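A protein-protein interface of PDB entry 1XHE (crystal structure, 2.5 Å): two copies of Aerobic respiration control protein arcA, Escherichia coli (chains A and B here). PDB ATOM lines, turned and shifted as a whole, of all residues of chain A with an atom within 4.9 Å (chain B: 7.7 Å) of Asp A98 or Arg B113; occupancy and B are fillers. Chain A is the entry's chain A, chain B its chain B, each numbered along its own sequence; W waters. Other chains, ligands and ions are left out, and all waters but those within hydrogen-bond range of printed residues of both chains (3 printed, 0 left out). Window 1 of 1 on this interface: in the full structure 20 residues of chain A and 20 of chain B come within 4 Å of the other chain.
Printed residues of chain A that touch a printed residue of chain B: Arg A70, Val A75, Ala A76, Lys A89, Leu A93, Ala A97, Asp A98, Asp A99 and Arg A113. Hydrophobic or aromatic side chains of chain A that line the printed part of chain B: Leu A93. Printed residues of chain B that touch a printed residue of chain A: Asp B99, Glu B109, Ile B112, Arg B113, Arg B115, Asn B116 and Arg B120. Among the printed residues, Asp or Glu carboxylates within 4 Å of a Lys or Arg side-chain nitrogen of the other chain: Lys A89 with Glu B109 (3.6 Å), Asp A98 with Arg B120 (2.7 Å), Asp A99 with Arg B113 (3.2 Å) and Arg A113 with Asp B99 (3.0 Å).
Water W3 lies within hydrogen-bond range of the side-chain amide nitrogen of Asn B116 (2.7 Å), the backbone carbonyl oxygen of Ala A97 (2.9 Å) and the backbone carbonyl oxygen of Asp A98 (3.4 Å). Water W2 lies within hydrogen-bond range of the side-chain carboxylate of Asp A99 (2.8 Å) and the guanidinium group of Arg B113 (3.2 Å). Water W1 lies within hydrogen-bond range of OD1 of Asp B99, O of Tyr B100, NH2 of Arg A113 and NH2 of Arg B113.
Arg B120 touches Ala A76. Glu B109 touches Leu A93 (CG to CD1, 3.8 Å). C of Leu A93 touches CG2 of Ile B112, 3.5 Å away. Leu A93 touches Arg B113. Arg B115 touches Leu A93 (NH2 to O, 3.9 Å). O of Asp A98 touches NH1 of Arg B113, at 3.96 Å.
Of the printed residues of chain B, Asp A98 touches Arg B113 (3.96 Å) and Arg B120 (2.7 Å). Printed residues of chain B within 4 Å of Ala A76: Arg B120. Printed residues of chain A within 4 Å of Ile B112: Leu A93 (3.5 Å). Leu B118 touches none of the printed residues of chain A. The nearest residue of chain A that does not touch Arg B113 is Lys A89 (4.05 Å).
NH1 of Arg A113 is in salt-bridge range of OD1 of Asp B99, 3.0 Å away. The guanidinium group (NH2) of Arg A70 lies close to the guanidinium group (NH2) of Arg B120, 3.1 Å away. The backbone carbonyl oxygen (O) of Val A75 is in hydrogen-bond range of the guanidinium group (NH2) of Arg B120. The side-chain amide nitrogen of Asn B116 lies within hydrogen-bond range of the backbone carbonyl oxygen of Leu A93 (3.2 Å). OD1 of Asp A99 lies within salt-bridge range of NH1 of Arg B113, 3.2 Å away. The side-chain amide nitrogen (ND2) of Asn B116 is in hydrogen-bond range of the backbone carbonyl oxygen (O) of Ala A97. The side-chain amino group of Lys A89 is in salt-bridge range of the side-chain carboxylate of Glu B109, 3.6 Å away. OD1 of Asp A98 is in salt-bridge range of NE of Arg B120.
Asp A98 touches Arg B113, but with the chains exchanged Arg A113 does not touch Asp B98 (4.1 Å). Asp A99 touches Arg B113, and with the chains exchanged Arg A113 touches Asp B99. Positions printed for both chains: 98, 99, 100, 113 and 117. Of the 14 pairs that touch across the chains among the printed residues, 2 have their exchanged pair printed and touching as well.
The guanidinium group of Arg B113 lies within salt-bridge range of the side-chain carboxylate of Glu B109, 2.7 Å away. The side-chain carboxylate (OD2) of Asp A99 lies within salt-bridge range of the guanidinium group (NH1) of Arg A113. The guanidinium group (NH2) of Arg A70 lies within salt-bridge range of the side-chain carboxylate (OD2) of Asp A98. The backbone carbonyl oxygen of Arg B115 lies within hydrogen-bond range of the side-chain hydroxyl of Ser B119 (3.4 Å). The side-chain carboxylate (OD2) of Asp B99 is in salt-bridge range of the guanidinium group (NH1) of Arg B113, at 2.9 Å. The guanidinium group (NH2) of Arg A70 lies within hydrogen-bond range of the backbone carbonyl oxygen (O) of Gly A96, 3.0 Å away.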
ATOM      1  N   ARG A  70      21.342 -23.870  17.926  1.00  0.00           N
ATOM      2  CA  ARG A  70      22.089 -23.127  16.906  1.00  0.00           C
ATOM      3  C   ARG A  70      23.590 -23.463  16.865  1.00  0.00           C
ATOM      4  O   ARG A  70      24.246 -23.217  15.860  1.00  0.00           O
ATOM      5  CB  ARG A  70      21.872 -21.612  17.041  1.00  0.00           C
ATOM      6  CG  ARG A  70      20.707 -21.102  16.208  1.00  0.00           C
ATOM      7  CD  ARG A  70      20.751 -21.550  14.762  1.00  0.00           C
ATOM      8  NE  ARG A  70      19.654 -21.020  13.959  1.00  0.00           N
ATOM      9  CZ  ARG A  70      18.682 -21.755  13.419  1.00  0.00           C
ATOM     10  NH1 ARG A  70      18.646 -23.078  13.596  1.00  0.00           N
ATOM     11  NH2 ARG A  70      17.738 -21.153  12.699  1.00  0.00           N
ATOM     12  N   VAL A  75      18.859 -25.560  11.201  1.00  0.00           N
ATOM     13  CA  VAL A  75      17.477 -25.847  10.809  1.00  0.00           C
ATOM     14  C   VAL A  75      16.549 -24.606  10.893  1.00  0.00           C
ATOM     15  O   VAL A  75      16.750 -23.710  11.702  1.00  0.00           O
ATOM     16  CB  VAL A  75      16.924 -27.048  11.645  1.00  0.00           C
ATOM     17  CG1 VAL A  75      17.003 -26.739  13.097  1.00  0.00           C
ATOM     18  CG2 VAL A  75      15.518 -27.389  11.263  1.00  0.00           C
ATOM     19  N   ALA A  76      15.546 -24.551  10.028  1.00  0.00           N
ATOM     20  CA  ALA A  76      14.611 -23.452  10.054  1.00  0.00           C
ATOM     21  C   ALA A  76      13.930 -23.412  11.432  1.00  0.00           C
ATOM     22  O   ALA A  76      13.448 -24.439  11.942  1.00  0.00           O
ATOM     23  CB  ALA A  76      13.607 -23.622   8.953  1.00  0.00           C
ATOM     24  N   LEU A  77      13.881 -22.218  12.016  1.00  0.00           N
ATOM     25  CA  LEU A  77      13.467 -22.050  13.385  1.00  0.00           C
ATOM     26  C   LEU A  77      12.493 -20.878  13.561  1.00  0.00           C
ATOM     27  O   LEU A  77      12.765 -19.788  13.103  1.00  0.00           O
ATOM     28  CB  LEU A  77      14.716 -21.890  14.292  1.00  0.00           C
ATOM     29  CG  LEU A  77      14.418 -21.482  15.749  1.00  0.00           C
ATOM     30  CD1 LEU A  77      13.755 -22.601  16.532  1.00  0.00           C
ATOM     31  CD2 LEU A  77      15.639 -20.975  16.484  1.00  0.00           C
ATOM     32  N   LYS A  89      11.889 -10.680  21.550  1.00  0.00           N
ATOM     33  CA  LYS A  89      11.765 -10.754  20.114  1.00  0.00           C
ATOM     34  C   LYS A  89      13.132 -10.536  19.484  1.00  0.00           C
ATOM     35  O   LYS A  89      13.568 -11.357  18.677  1.00  0.00           O
ATOM     36  CB  LYS A  89      10.721  -9.746  19.620  1.00  0.00           C
ATOM     37  CG  LYS A  89      10.959  -9.175  18.221  1.00  0.00           C
ATOM     38  CD  LYS A  89       9.907  -9.619  17.275  1.00  0.00           C
ATOM     39  CE  LYS A  89       9.091  -8.445  16.797  1.00  0.00           C
ATOM     40  NZ  LYS A  89       7.881  -8.887  15.951  1.00  0.00           N
ATOM     41  N   LEU A  93      15.601 -13.310  17.560  1.00  0.00           N
ATOM     42  CA  LEU A  93      16.134 -13.199  16.217  1.00  0.00           C
ATOM     43  C   LEU A  93      17.666 -13.173  16.288  1.00  0.00           C
ATOM     44  O   LEU A  93      18.351 -13.850  15.530  1.00  0.00           O
ATOM     45  CB  LEU A  93      15.538 -12.003  15.487  1.00  0.00           C
ATOM     46  CG  LEU A  93      14.011 -11.915  15.416  1.00  0.00           C
ATOM     47  CD1 LEU A  93      13.549 -10.503  15.061  1.00  0.00           C
ATOM     48  CD2 LEU A  93      13.455 -12.965  14.412  1.00  0.00           C
ATOM     49  N   GLY A  96      19.317 -16.403  16.153  1.00  0.00           N
ATOM     50  CA  GLY A  96      19.198 -17.084  14.889  1.00  0.00           C
ATOM     51  C   GLY A  96      17.830 -17.578  14.462  1.00  0.00           C
ATOM     52  O   GLY A  96      17.736 -18.227  13.424  1.00  0.00           O
ATOM     53  N   ALA A  97      16.778 -17.316  15.236  1.00  0.00           N
ATOM     54  CA  ALA A  97      15.431 -17.670  14.781  1.00  0.00           C
ATOM     55  C   ALA A  97      15.165 -16.954  13.465  1.00  0.00           C
ATOM     56  O   ALA A  97      15.498 -15.770  13.299  1.00  0.00           O
ATOM     57  CB  ALA A  97      14.361 -17.247  15.841  1.00  0.00           C
ATOM     58  N   ASP A  98      14.541 -17.644  12.536  1.00  0.00           N
ATOM     59  CA  ASP A  98      14.132 -17.016  11.278  1.00  0.00           C
ATOM     60  C   ASP A  98      12.887 -16.184  11.441  1.00  0.00           C
ATOM     61  O   ASP A  98      12.661 -15.235  10.717  1.00  0.00           O
ATOM     62  CB  ASP A  98      13.889 -18.090  10.239  1.00  0.00           C
ATOM     63  CG  ASP A  98      15.124 -18.844   9.952  1.00  0.00           C
ATOM     64  OD1 ASP A  98      16.082 -18.342   9.303  1.00  0.00           O
ATOM     65  OD2 ASP A  98      15.228 -19.975  10.440  1.00  0.00           O
ATOM     66  N   ASP A  99      12.058 -16.533  12.392  1.00  0.00           N
ATOM     67  CA  ASP A  99      10.944 -15.678  12.637  1.00  0.00           C
ATOM     68  C   ASP A  99      10.527 -15.731  14.065  1.00  0.00           C
ATOM     69  O   ASP A  99      10.981 -16.580  14.825  1.00  0.00           O
ATOM     70  CB  ASP A  99       9.798 -16.040  11.741  1.00  0.00           C
ATOM     71  CG  ASP A  99       9.107 -14.823  11.204  1.00  0.00           C
ATOM     72  OD1 ASP A  99       8.788 -13.867  12.002  1.00  0.00           O
ATOM     73  OD2 ASP A  99       8.873 -14.747   9.966  1.00  0.00           O
ATOM     74  N   TYR A 100       9.670 -14.803  14.431  1.00  0.00           N
ATOM     75  CA  TYR A 100       9.289 -14.631  15.807  1.00  0.00           C
ATOM     76  C   TYR A 100       7.828 -14.337  15.768  1.00  0.00           C
ATOM     77  O   TYR A 100       7.419 -13.325  15.226  1.00  0.00           O
ATOM     78  CB  TYR A 100      10.026 -13.435  16.413  1.00  0.00           C
ATOM     79  CG  TYR A 100       9.920 -13.453  17.898  1.00  0.00           C
ATOM     80  CD1 TYR A 100       8.843 -12.849  18.523  1.00  0.00           C
ATOM     81  CD2 TYR A 100      10.881 -14.137  18.701  1.00  0.00           C
ATOM     82  CE1 TYR A 100       8.696 -12.898  19.914  1.00  0.00           C
ATOM     83  CE2 TYR A 100      10.744 -14.188  20.101  1.00  0.00           C
ATOM     84  CZ  TYR A 100       9.639 -13.572  20.690  1.00  0.00           C
ATOM     85  OH  TYR A 100       9.434 -13.586  22.050  1.00  0.00           O
ATOM     86  N   ARG A 113       4.608 -17.986   5.775  1.00  0.00           N
ATOM     87  CA  ARG A 113       5.985 -17.802   6.224  1.00  0.00           C
ATOM     88  C   ARG A 113       6.683 -19.152   6.280  1.00  0.00           C
ATOM     89  O   ARG A 113       7.820 -19.290   5.801  1.00  0.00           O
ATOM     90  CB  ARG A 113       6.037 -17.154   7.588  1.00  0.00           C
ATOM     91  CG  ARG A 113       5.754 -15.667   7.606  1.00  0.00           C
ATOM     92  CD  ARG A 113       5.960 -15.034   8.973  1.00  0.00           C
ATOM     93  NE  ARG A 113       5.531 -13.637   9.035  1.00  0.00           N
ATOM     94  CZ  ARG A 113       6.351 -12.603   8.836  1.00  0.00           C
ATOM     95  NH1 ARG A 113       7.645 -12.834   8.566  1.00  0.00           N
ATOM     96  NH2 ARG A 113       5.880 -11.350   8.879  1.00  0.00           N
ATOM     97  N   LEU A 117       9.881 -20.083   3.897  1.00  0.00           N
ATOM     98  CA  LEU A 117      11.146 -20.373   4.543  1.00  0.00           C
ATOM     99  C   LEU A 117      11.558 -21.793   4.151  1.00  0.00           C
ATOM    100  O   LEU A 117      12.707 -22.058   3.827  1.00  0.00           O
ATOM    101  CB  LEU A 117      11.008 -20.235   6.053  1.00  0.00           C
ATOM    102  CG  LEU A 117      12.252 -20.543   6.897  1.00  0.00           C
ATOM    103  CD1 LEU A 117      13.446 -19.640   6.534  1.00  0.00           C
ATOM    104  CD2 LEU A 117      11.920 -20.460   8.424  1.00  0.00           C
ATOM    105  N   PHE B  23      21.685   0.467   6.817  1.00  0.00           N
ATOM    106  CA  PHE B  23      22.461  -0.630   6.222  1.00  0.00           C
ATOM    107  C   PHE B  23      23.887  -0.293   5.944  1.00  0.00           C
ATOM    108  O   PHE B  23      24.721  -1.182   5.860  1.00  0.00           O
ATOM    109  CB  PHE B  23      21.804  -1.242   4.969  1.00  0.00           C
ATOM    110  CG  PHE B  23      20.579  -2.018   5.273  1.00  0.00           C
ATOM    111  CD1 PHE B  23      20.667  -3.352   5.675  1.00  0.00           C
ATOM    112  CD2 PHE B  23      19.331  -1.406   5.242  1.00  0.00           C
ATOM    113  CE1 PHE B  23      19.547  -4.076   5.992  1.00  0.00           C
ATOM    114  CE2 PHE B  23      18.189  -2.126   5.557  1.00  0.00           C
ATOM    115  CZ  PHE B  23      18.305  -3.471   5.923  1.00  0.00           C
ATOM    116  N   TYR B  28      26.980  -2.769   4.418  1.00  0.00           N
ATOM    117  CA  TYR B  28      26.382  -3.152   3.135  1.00  0.00           C
ATOM    118  C   TYR B  28      26.631  -2.055   2.108  1.00  0.00           C
ATOM    119  O   TYR B  28      26.661  -0.879   2.456  1.00  0.00           O
ATOM    120  CB  TYR B  28      24.845  -3.307   3.251  1.00  0.00           C
ATOM    121  CG  TYR B  28      24.391  -4.429   4.148  1.00  0.00           C
ATOM    122  CD1 TYR B  28      25.309  -5.137   4.915  1.00  0.00           C
ATOM    123  CD2 TYR B  28      23.051  -4.816   4.216  1.00  0.00           C
ATOM    124  CE1 TYR B  28      24.909  -6.170   5.740  1.00  0.00           C
ATOM    125  CE2 TYR B  28      22.646  -5.877   5.048  1.00  0.00           C
ATOM    126  CZ  TYR B  28      23.582  -6.515   5.810  1.00  0.00           C
ATOM    127  OH  TYR B  28      23.259  -7.557   6.630  1.00  0.00           O
ATOM    128  N   LEU B  50      19.583  -8.390  -1.586  1.00  0.00           N
ATOM    129  CA  LEU B  50      18.380  -8.142  -0.857  1.00  0.00           C
ATOM    130  C   LEU B  50      17.668  -6.905  -1.395  1.00  0.00           C
ATOM    131  O   LEU B  50      18.295  -5.872  -1.649  1.00  0.00           O
ATOM    132  CB  LEU B  50      18.715  -7.944   0.611  1.00  0.00           C
ATOM    133  CG  LEU B  50      17.614  -7.552   1.617  1.00  0.00           C
ATOM    134  CD1 LEU B  50      16.518  -8.612   1.743  1.00  0.00           C
ATOM    135  CD2 LEU B  50      18.291  -7.287   2.985  1.00  0.00           C
ATOM    136  N   MET B  78      12.221  -8.106   1.377  1.00  0.00           N
ATOM    137  CA  MET B  78      11.351  -7.671   2.489  1.00  0.00           C
ATOM    138  C   MET B  78      10.536  -6.469   2.066  1.00  0.00           C
ATOM    139  O   MET B  78      11.046  -5.567   1.421  1.00  0.00           O
ATOM    140  CB  MET B  78      12.131  -7.302   3.758  1.00  0.00           C
ATOM    141  CG  MET B  78      12.983  -8.399   4.283  1.00  0.00           C
ATOM    142  SD  MET B  78      14.098  -7.790   5.550  1.00  0.00           S
ATOM    143  CE  MET B  78      14.993  -9.293   5.886  1.00  0.00           C
ATOM    144  N   ASP B  98      10.033 -12.525   1.807  1.00  0.00           N
ATOM    145  CA  ASP B  98      10.526 -13.269   2.955  1.00  0.00           C
ATOM    146  C   ASP B  98      10.139 -12.621   4.274  1.00  0.00           C
ATOM    147  O   ASP B  98      10.095 -13.262   5.303  1.00  0.00           O
ATOM    148  CB  ASP B  98      12.025 -13.368   2.886  1.00  0.00           C
ATOM    149  CG  ASP B  98      12.468 -14.007   1.656  1.00  0.00           C
ATOM    150  OD1 ASP B  98      12.426 -15.259   1.611  1.00  0.00           O
ATOM    151  OD2 ASP B  98      12.850 -13.331   0.677  1.00  0.00           O
ATOM    152  N   ASP B  99       9.890 -11.330   4.241  1.00  0.00           N
ATOM    153  CA  ASP B  99       9.443 -10.654   5.423  1.00  0.00           C
ATOM    154  C   ASP B  99       8.665  -9.412   5.089  1.00  0.00           C
ATOM    155  O   ASP B  99       8.670  -8.922   3.941  1.00  0.00           O
ATOM    156  CB  ASP B  99      10.613 -10.286   6.296  1.00  0.00           C
ATOM    157  CG  ASP B  99      10.354 -10.626   7.743  1.00  0.00           C
ATOM    158  OD1 ASP B  99       9.221 -10.290   8.260  1.00  0.00           O
ATOM    159  OD2 ASP B  99      11.221 -11.263   8.417  1.00  0.00           O
ATOM    160  N   TYR B 100       8.009  -8.909   6.122  1.00  0.00           N
ATOM    161  CA  TYR B 100       7.102  -7.796   6.028  1.00  0.00           C
ATOM    162  C   TYR B 100       7.346  -6.960   7.276  1.00  0.00           C
ATOM    163  O   TYR B 100       7.158  -7.416   8.403  1.00  0.00           O
ATOM    164  CB  TYR B 100       5.661  -8.311   6.010  1.00  0.00           C
ATOM    165  CG  TYR B 100       4.709  -7.257   5.550  1.00  0.00           C
ATOM    166  CD1 TYR B 100       4.225  -6.302   6.445  1.00  0.00           C
ATOM    167  CD2 TYR B 100       4.310  -7.178   4.193  1.00  0.00           C
ATOM    168  CE1 TYR B 100       3.354  -5.298   6.022  1.00  0.00           C
ATOM    169  CE2 TYR B 100       3.447  -6.165   3.753  1.00  0.00           C
ATOM    170  CZ  TYR B 100       2.983  -5.226   4.681  1.00  0.00           C
ATOM    171  OH  TYR B 100       2.141  -4.213   4.280  1.00  0.00           O
ATOM    172  N   ILE B 101       7.799  -5.739   7.106  1.00  0.00           N
ATOM    173  CA  ILE B 101       8.032  -4.930   8.289  1.00  0.00           C
ATOM    174  C   ILE B 101       7.273  -3.591   8.272  1.00  0.00           C
ATOM    175  O   ILE B 101       7.240  -2.885   7.255  1.00  0.00           O
ATOM    176  CB  ILE B 101       9.572  -4.834   8.590  1.00  0.00           C
ATOM    177  CG1 ILE B 101      10.118  -6.266   8.852  1.00  0.00           C
ATOM    178  CG2 ILE B 101       9.844  -3.913   9.823  1.00  0.00           C
ATOM    179  CD1 ILE B 101      11.636  -6.505   8.563  1.00  0.00           C
ATOM    180  N   PRO B 107      15.358  -0.550  14.061  1.00  0.00           N
ATOM    181  CA  PRO B 107      16.457  -0.793  13.129  1.00  0.00           C
ATOM    182  C   PRO B 107      17.138  -2.099  13.442  1.00  0.00           C
ATOM    183  O   PRO B 107      17.574  -2.794  12.501  1.00  0.00           O
ATOM    184  CB  PRO B 107      17.422   0.355  13.412  1.00  0.00           C
ATOM    185  CG  PRO B 107      16.529   1.490  13.996  1.00  0.00           C
ATOM    186  CD  PRO B 107      15.411   0.785  14.696  1.00  0.00           C
ATOM    187  N   ARG B 108      17.267  -2.442  14.724  1.00  0.00           N
ATOM    188  CA  ARG B 108      17.953  -3.697  15.070  1.00  0.00           C
ATOM    189  C   ARG B 108      17.188  -4.896  14.592  1.00  0.00           C
ATOM    190  O   ARG B 108      17.780  -5.850  14.130  1.00  0.00           O
ATOM    191  CB  ARG B 108      18.211  -3.851  16.568  1.00  0.00           C
ATOM    192  CG  ARG B 108      18.996  -2.729  17.171  1.00  0.00           C
ATOM    193  CD  ARG B 108      20.412  -2.639  16.702  1.00  0.00           C
ATOM    194  NE  ARG B 108      21.013  -1.567  17.479  1.00  0.00           N
ATOM    195  CZ  ARG B 108      21.943  -0.727  17.052  1.00  0.00           C
ATOM    196  NH1 ARG B 108      22.441  -0.852  15.827  1.00  0.00           N
ATOM    197  NH2 ARG B 108      22.383   0.231  17.869  1.00  0.00           N
ATOM    198  N   GLU B 109      15.874  -4.856  14.684  1.00  0.00           N
ATOM    199  CA  GLU B 109      15.105  -6.000  14.207  1.00  0.00           C
ATOM    200  C   GLU B 109      15.316  -6.197  12.709  1.00  0.00           C
ATOM    201  O   GLU B 109      15.459  -7.334  12.229  1.00  0.00           O
ATOM    202  CB  GLU B 109      13.615  -5.849  14.498  1.00  0.00           C
ATOM    203  CG  GLU B 109      12.841  -7.009  13.894  1.00  0.00           C
ATOM    204  CD  GLU B 109      11.354  -6.996  14.210  1.00  0.00           C
ATOM    205  OE1 GLU B 109      10.921  -6.034  14.889  1.00  0.00           O
ATOM    206  OE2 GLU B 109      10.636  -7.958  13.795  1.00  0.00           O
ATOM    207  N   LEU B 110      15.337  -5.079  11.991  1.00  0.00           N
ATOM    208  CA  LEU B 110      15.524  -5.034  10.555  1.00  0.00           C
ATOM    209  C   LEU B 110      16.881  -5.616  10.122  1.00  0.00           C
ATOM    210  O   LEU B 110      16.961  -6.501   9.259  1.00  0.00           O
ATOM    211  CB  LEU B 110      15.358  -3.587  10.079  1.00  0.00           C
ATOM    212  CG  LEU B 110      15.537  -3.327   8.580  1.00  0.00           C
ATOM    213  CD1 LEU B 110      14.646  -4.288   7.831  1.00  0.00           C
ATOM    214  CD2 LEU B 110      15.235  -1.897   8.177  1.00  0.00           C
ATOM    215  N   THR B 111      17.954  -5.166  10.739  1.00  0.00           N
ATOM    216  CA  THR B 111      19.259  -5.673  10.323  1.00  0.00           C
ATOM    217  C   THR B 111      19.525  -7.064  10.833  1.00  0.00           C
ATOM    218  O   THR B 111      20.235  -7.804  10.192  1.00  0.00           O
ATOM    219  CB  THR B 111      20.388  -4.717  10.760  1.00  0.00           C
ATOM    220  OG1 THR B 111      20.285  -4.523  12.176  1.00  0.00           O
ATOM    221  CG2 THR B 111      20.158  -3.276  10.186  1.00  0.00           C
ATOM    222  N   ILE B 112      19.001  -7.453  11.993  1.00  0.00           N
ATOM    223  CA  ILE B 112      19.152  -8.849  12.358  1.00  0.00           C
ATOM    224  C   ILE B 112      18.330  -9.758  11.415  1.00  0.00           C
ATOM    225  O   ILE B 112      18.827 -10.803  11.006  1.00  0.00           O
ATOM    226  CB  ILE B 112      18.774  -9.086  13.824  1.00  0.00           C
ATOM    227  CG1 ILE B 112      19.681  -8.283  14.745  1.00  0.00           C
ATOM    228  CG2 ILE B 112      18.767 -10.620  14.159  1.00  0.00           C
ATOM    229  CD1 ILE B 112      19.179  -8.244  16.166  1.00  0.00           C
ATOM    230  N   ARG B 113      17.094  -9.382  11.048  1.00  0.00           N
ATOM    231  CA  ARG B 113      16.343 -10.235  10.109  1.00  0.00           C
ATOM    232  C   ARG B 113      17.052 -10.310   8.755  1.00  0.00           C
ATOM    233  O   ARG B 113      17.072 -11.386   8.122  1.00  0.00           O
ATOM    234  CB  ARG B 113      14.910  -9.756   9.859  1.00  0.00           C
ATOM    235  CG  ARG B 113      13.992  -9.825  11.005  1.00  0.00           C
ATOM    236  CD  ARG B 113      12.590  -9.431  10.686  1.00  0.00           C
ATOM    237  NE  ARG B 113      11.688  -9.586  11.847  1.00  0.00           N
ATOM    238  CZ  ARG B 113      10.940 -10.667  12.077  1.00  0.00           C
ATOM    239  NH1 ARG B 113      10.987 -11.687  11.244  1.00  0.00           N
ATOM    240  NH2 ARG B 113      10.148 -10.728  13.149  1.00  0.00           N
ATOM    241  N   ALA B 114      17.609  -9.178   8.293  1.00  0.00           N
ATOM    242  CA  ALA B 114      18.361  -9.181   7.023  1.00  0.00           C
ATOM    243  C   ALA B 114      19.564 -10.086   7.156  1.00  0.00           C
ATOM    244  O   ALA B 114      19.831 -10.891   6.273  1.00  0.00           O
ATOM    245  CB  ALA B 114      18.805  -7.761   6.625  1.00  0.00           C
ATOM    246  N   ARG B 115      20.288  -9.985   8.271  1.00  0.00           N
ATOM    247  CA  ARG B 115      21.441 -10.837   8.432  1.00  0.00           C
ATOM    248  C   ARG B 115      21.037 -12.292   8.419  1.00  0.00           C
ATOM    249  O   ARG B 115      21.647 -13.083   7.718  1.00  0.00           O
ATOM    250  CB  ARG B 115      22.277 -10.474   9.660  1.00  0.00           C
ATOM    251  CG  ARG B 115      23.474 -11.396   9.902  1.00  0.00           C
ATOM    252  CD  ARG B 115      23.971 -11.437  11.366  1.00  0.00           C
ATOM    253  NE  ARG B 115      23.121 -12.354  12.172  1.00  0.00           N
ATOM    254  CZ  ARG B 115      22.666 -12.133  13.437  1.00  0.00           C
ATOM    255  NH1 ARG B 115      23.009 -10.995  14.055  1.00  0.00           N
ATOM    256  NH2 ARG B 115      21.881 -13.069  14.066  1.00  0.00           N
ATOM    257  N   ASN B 116      19.989 -12.688   9.133  1.00  0.00           N
ATOM    258  CA  ASN B 116      19.693 -14.131   9.148  1.00  0.00           C
ATOM    259  C   ASN B 116      19.284 -14.641   7.774  1.00  0.00           C
ATOM    260  O   ASN B 116      19.631 -15.735   7.387  1.00  0.00           O
ATOM    261  CB  ASN B 116      18.571 -14.458  10.135  1.00  0.00           C
ATOM    262  CG  ASN B 116      18.977 -14.244  11.586  1.00  0.00           C
ATOM    263  OD1 ASN B 116      20.155 -14.453  11.990  1.00  0.00           O
ATOM    264  ND2 ASN B 116      18.005 -13.839  12.382  1.00  0.00           N
ATOM    265  N   LEU B 117      18.486 -13.843   7.075  1.00  0.00           N
ATOM    266  CA  LEU B 117      17.986 -14.175   5.760  1.00  0.00           C
ATOM    267  C   LEU B 117      19.163 -14.256   4.744  1.00  0.00           C
ATOM    268  O   LEU B 117      19.310 -15.230   4.008  1.00  0.00           O
ATOM    269  CB  LEU B 117      16.935 -13.153   5.341  1.00  0.00           C
ATOM    270  CG  LEU B 117      16.346 -13.269   3.943  1.00  0.00           C
ATOM    271  CD1 LEU B 117      15.699 -14.650   3.799  1.00  0.00           C
ATOM    272  CD2 LEU B 117      15.342 -12.129   3.698  1.00  0.00           C
ATOM    273  N   LEU B 118      20.038 -13.259   4.773  1.00  0.00           N
ATOM    274  CA  LEU B 118      21.242 -13.276   3.939  1.00  0.00           C
ATOM    275  C   LEU B 118      22.131 -14.484   4.243  1.00  0.00           C
ATOM    276  O   LEU B 118      22.802 -14.980   3.362  1.00  0.00           O
ATOM    277  CB  LEU B 118      22.023 -11.971   4.113  1.00  0.00           C
ATOM    278  CG  LEU B 118      21.798 -10.904   3.052  1.00  0.00           C
ATOM    279  CD1 LEU B 118      20.539 -11.167   2.390  1.00  0.00           C
ATOM    280  CD2 LEU B 118      21.811  -9.534   3.627  1.00  0.00           C
ATOM    281  N   SER B 119      22.131 -14.973   5.479  1.00  0.00           N
ATOM    282  CA  SER B 119      22.954 -16.130   5.822  1.00  0.00           C
ATOM    283  C   SER B 119      22.468 -17.380   5.119  1.00  0.00           C
ATOM    284  O   SER B 119      23.269 -18.227   4.763  1.00  0.00           O
ATOM    285  CB  SER B 119      22.963 -16.375   7.325  1.00  0.00           C
ATOM    286  OG  SER B 119      23.982 -15.583   7.922  1.00  0.00           O
ATOM    287  N   ARG B 120      21.155 -17.469   4.922  1.00  0.00           N
ATOM    288  CA  ARG B 120      20.545 -18.547   4.174  1.00  0.00           C
ATOM    289  C   ARG B 120      20.638 -18.394   2.655  1.00  0.00           C
ATOM    290  O   ARG B 120      20.745 -19.401   1.962  1.00  0.00           O
ATOM    291  CB  ARG B 120      19.078 -18.671   4.555  1.00  0.00           C
ATOM    292  CG  ARG B 120      18.883 -18.919   6.032  1.00  0.00           C
ATOM    293  CD  ARG B 120      17.672 -19.714   6.317  1.00  0.00           C
ATOM    294  NE  ARG B 120      17.467 -19.986   7.737  1.00  0.00           N
ATOM    295  CZ  ARG B 120      17.901 -21.080   8.367  1.00  0.00           C
ATOM    296  NH1 ARG B 120      18.613 -21.985   7.712  1.00  0.00           N
ATOM    297  NH2 ARG B 120      17.618 -21.266   9.652  1.00  0.00           N
HETATM  298  O   HOH W   1       8.111  -9.497  10.685  1.00  0.00           O
HETATM  299  O   HOH W   2       7.192 -11.593  12.151  1.00  0.00           O
HETATM  300  O   HOH W   3      15.443 -13.481  11.460  1.00  0.00           O
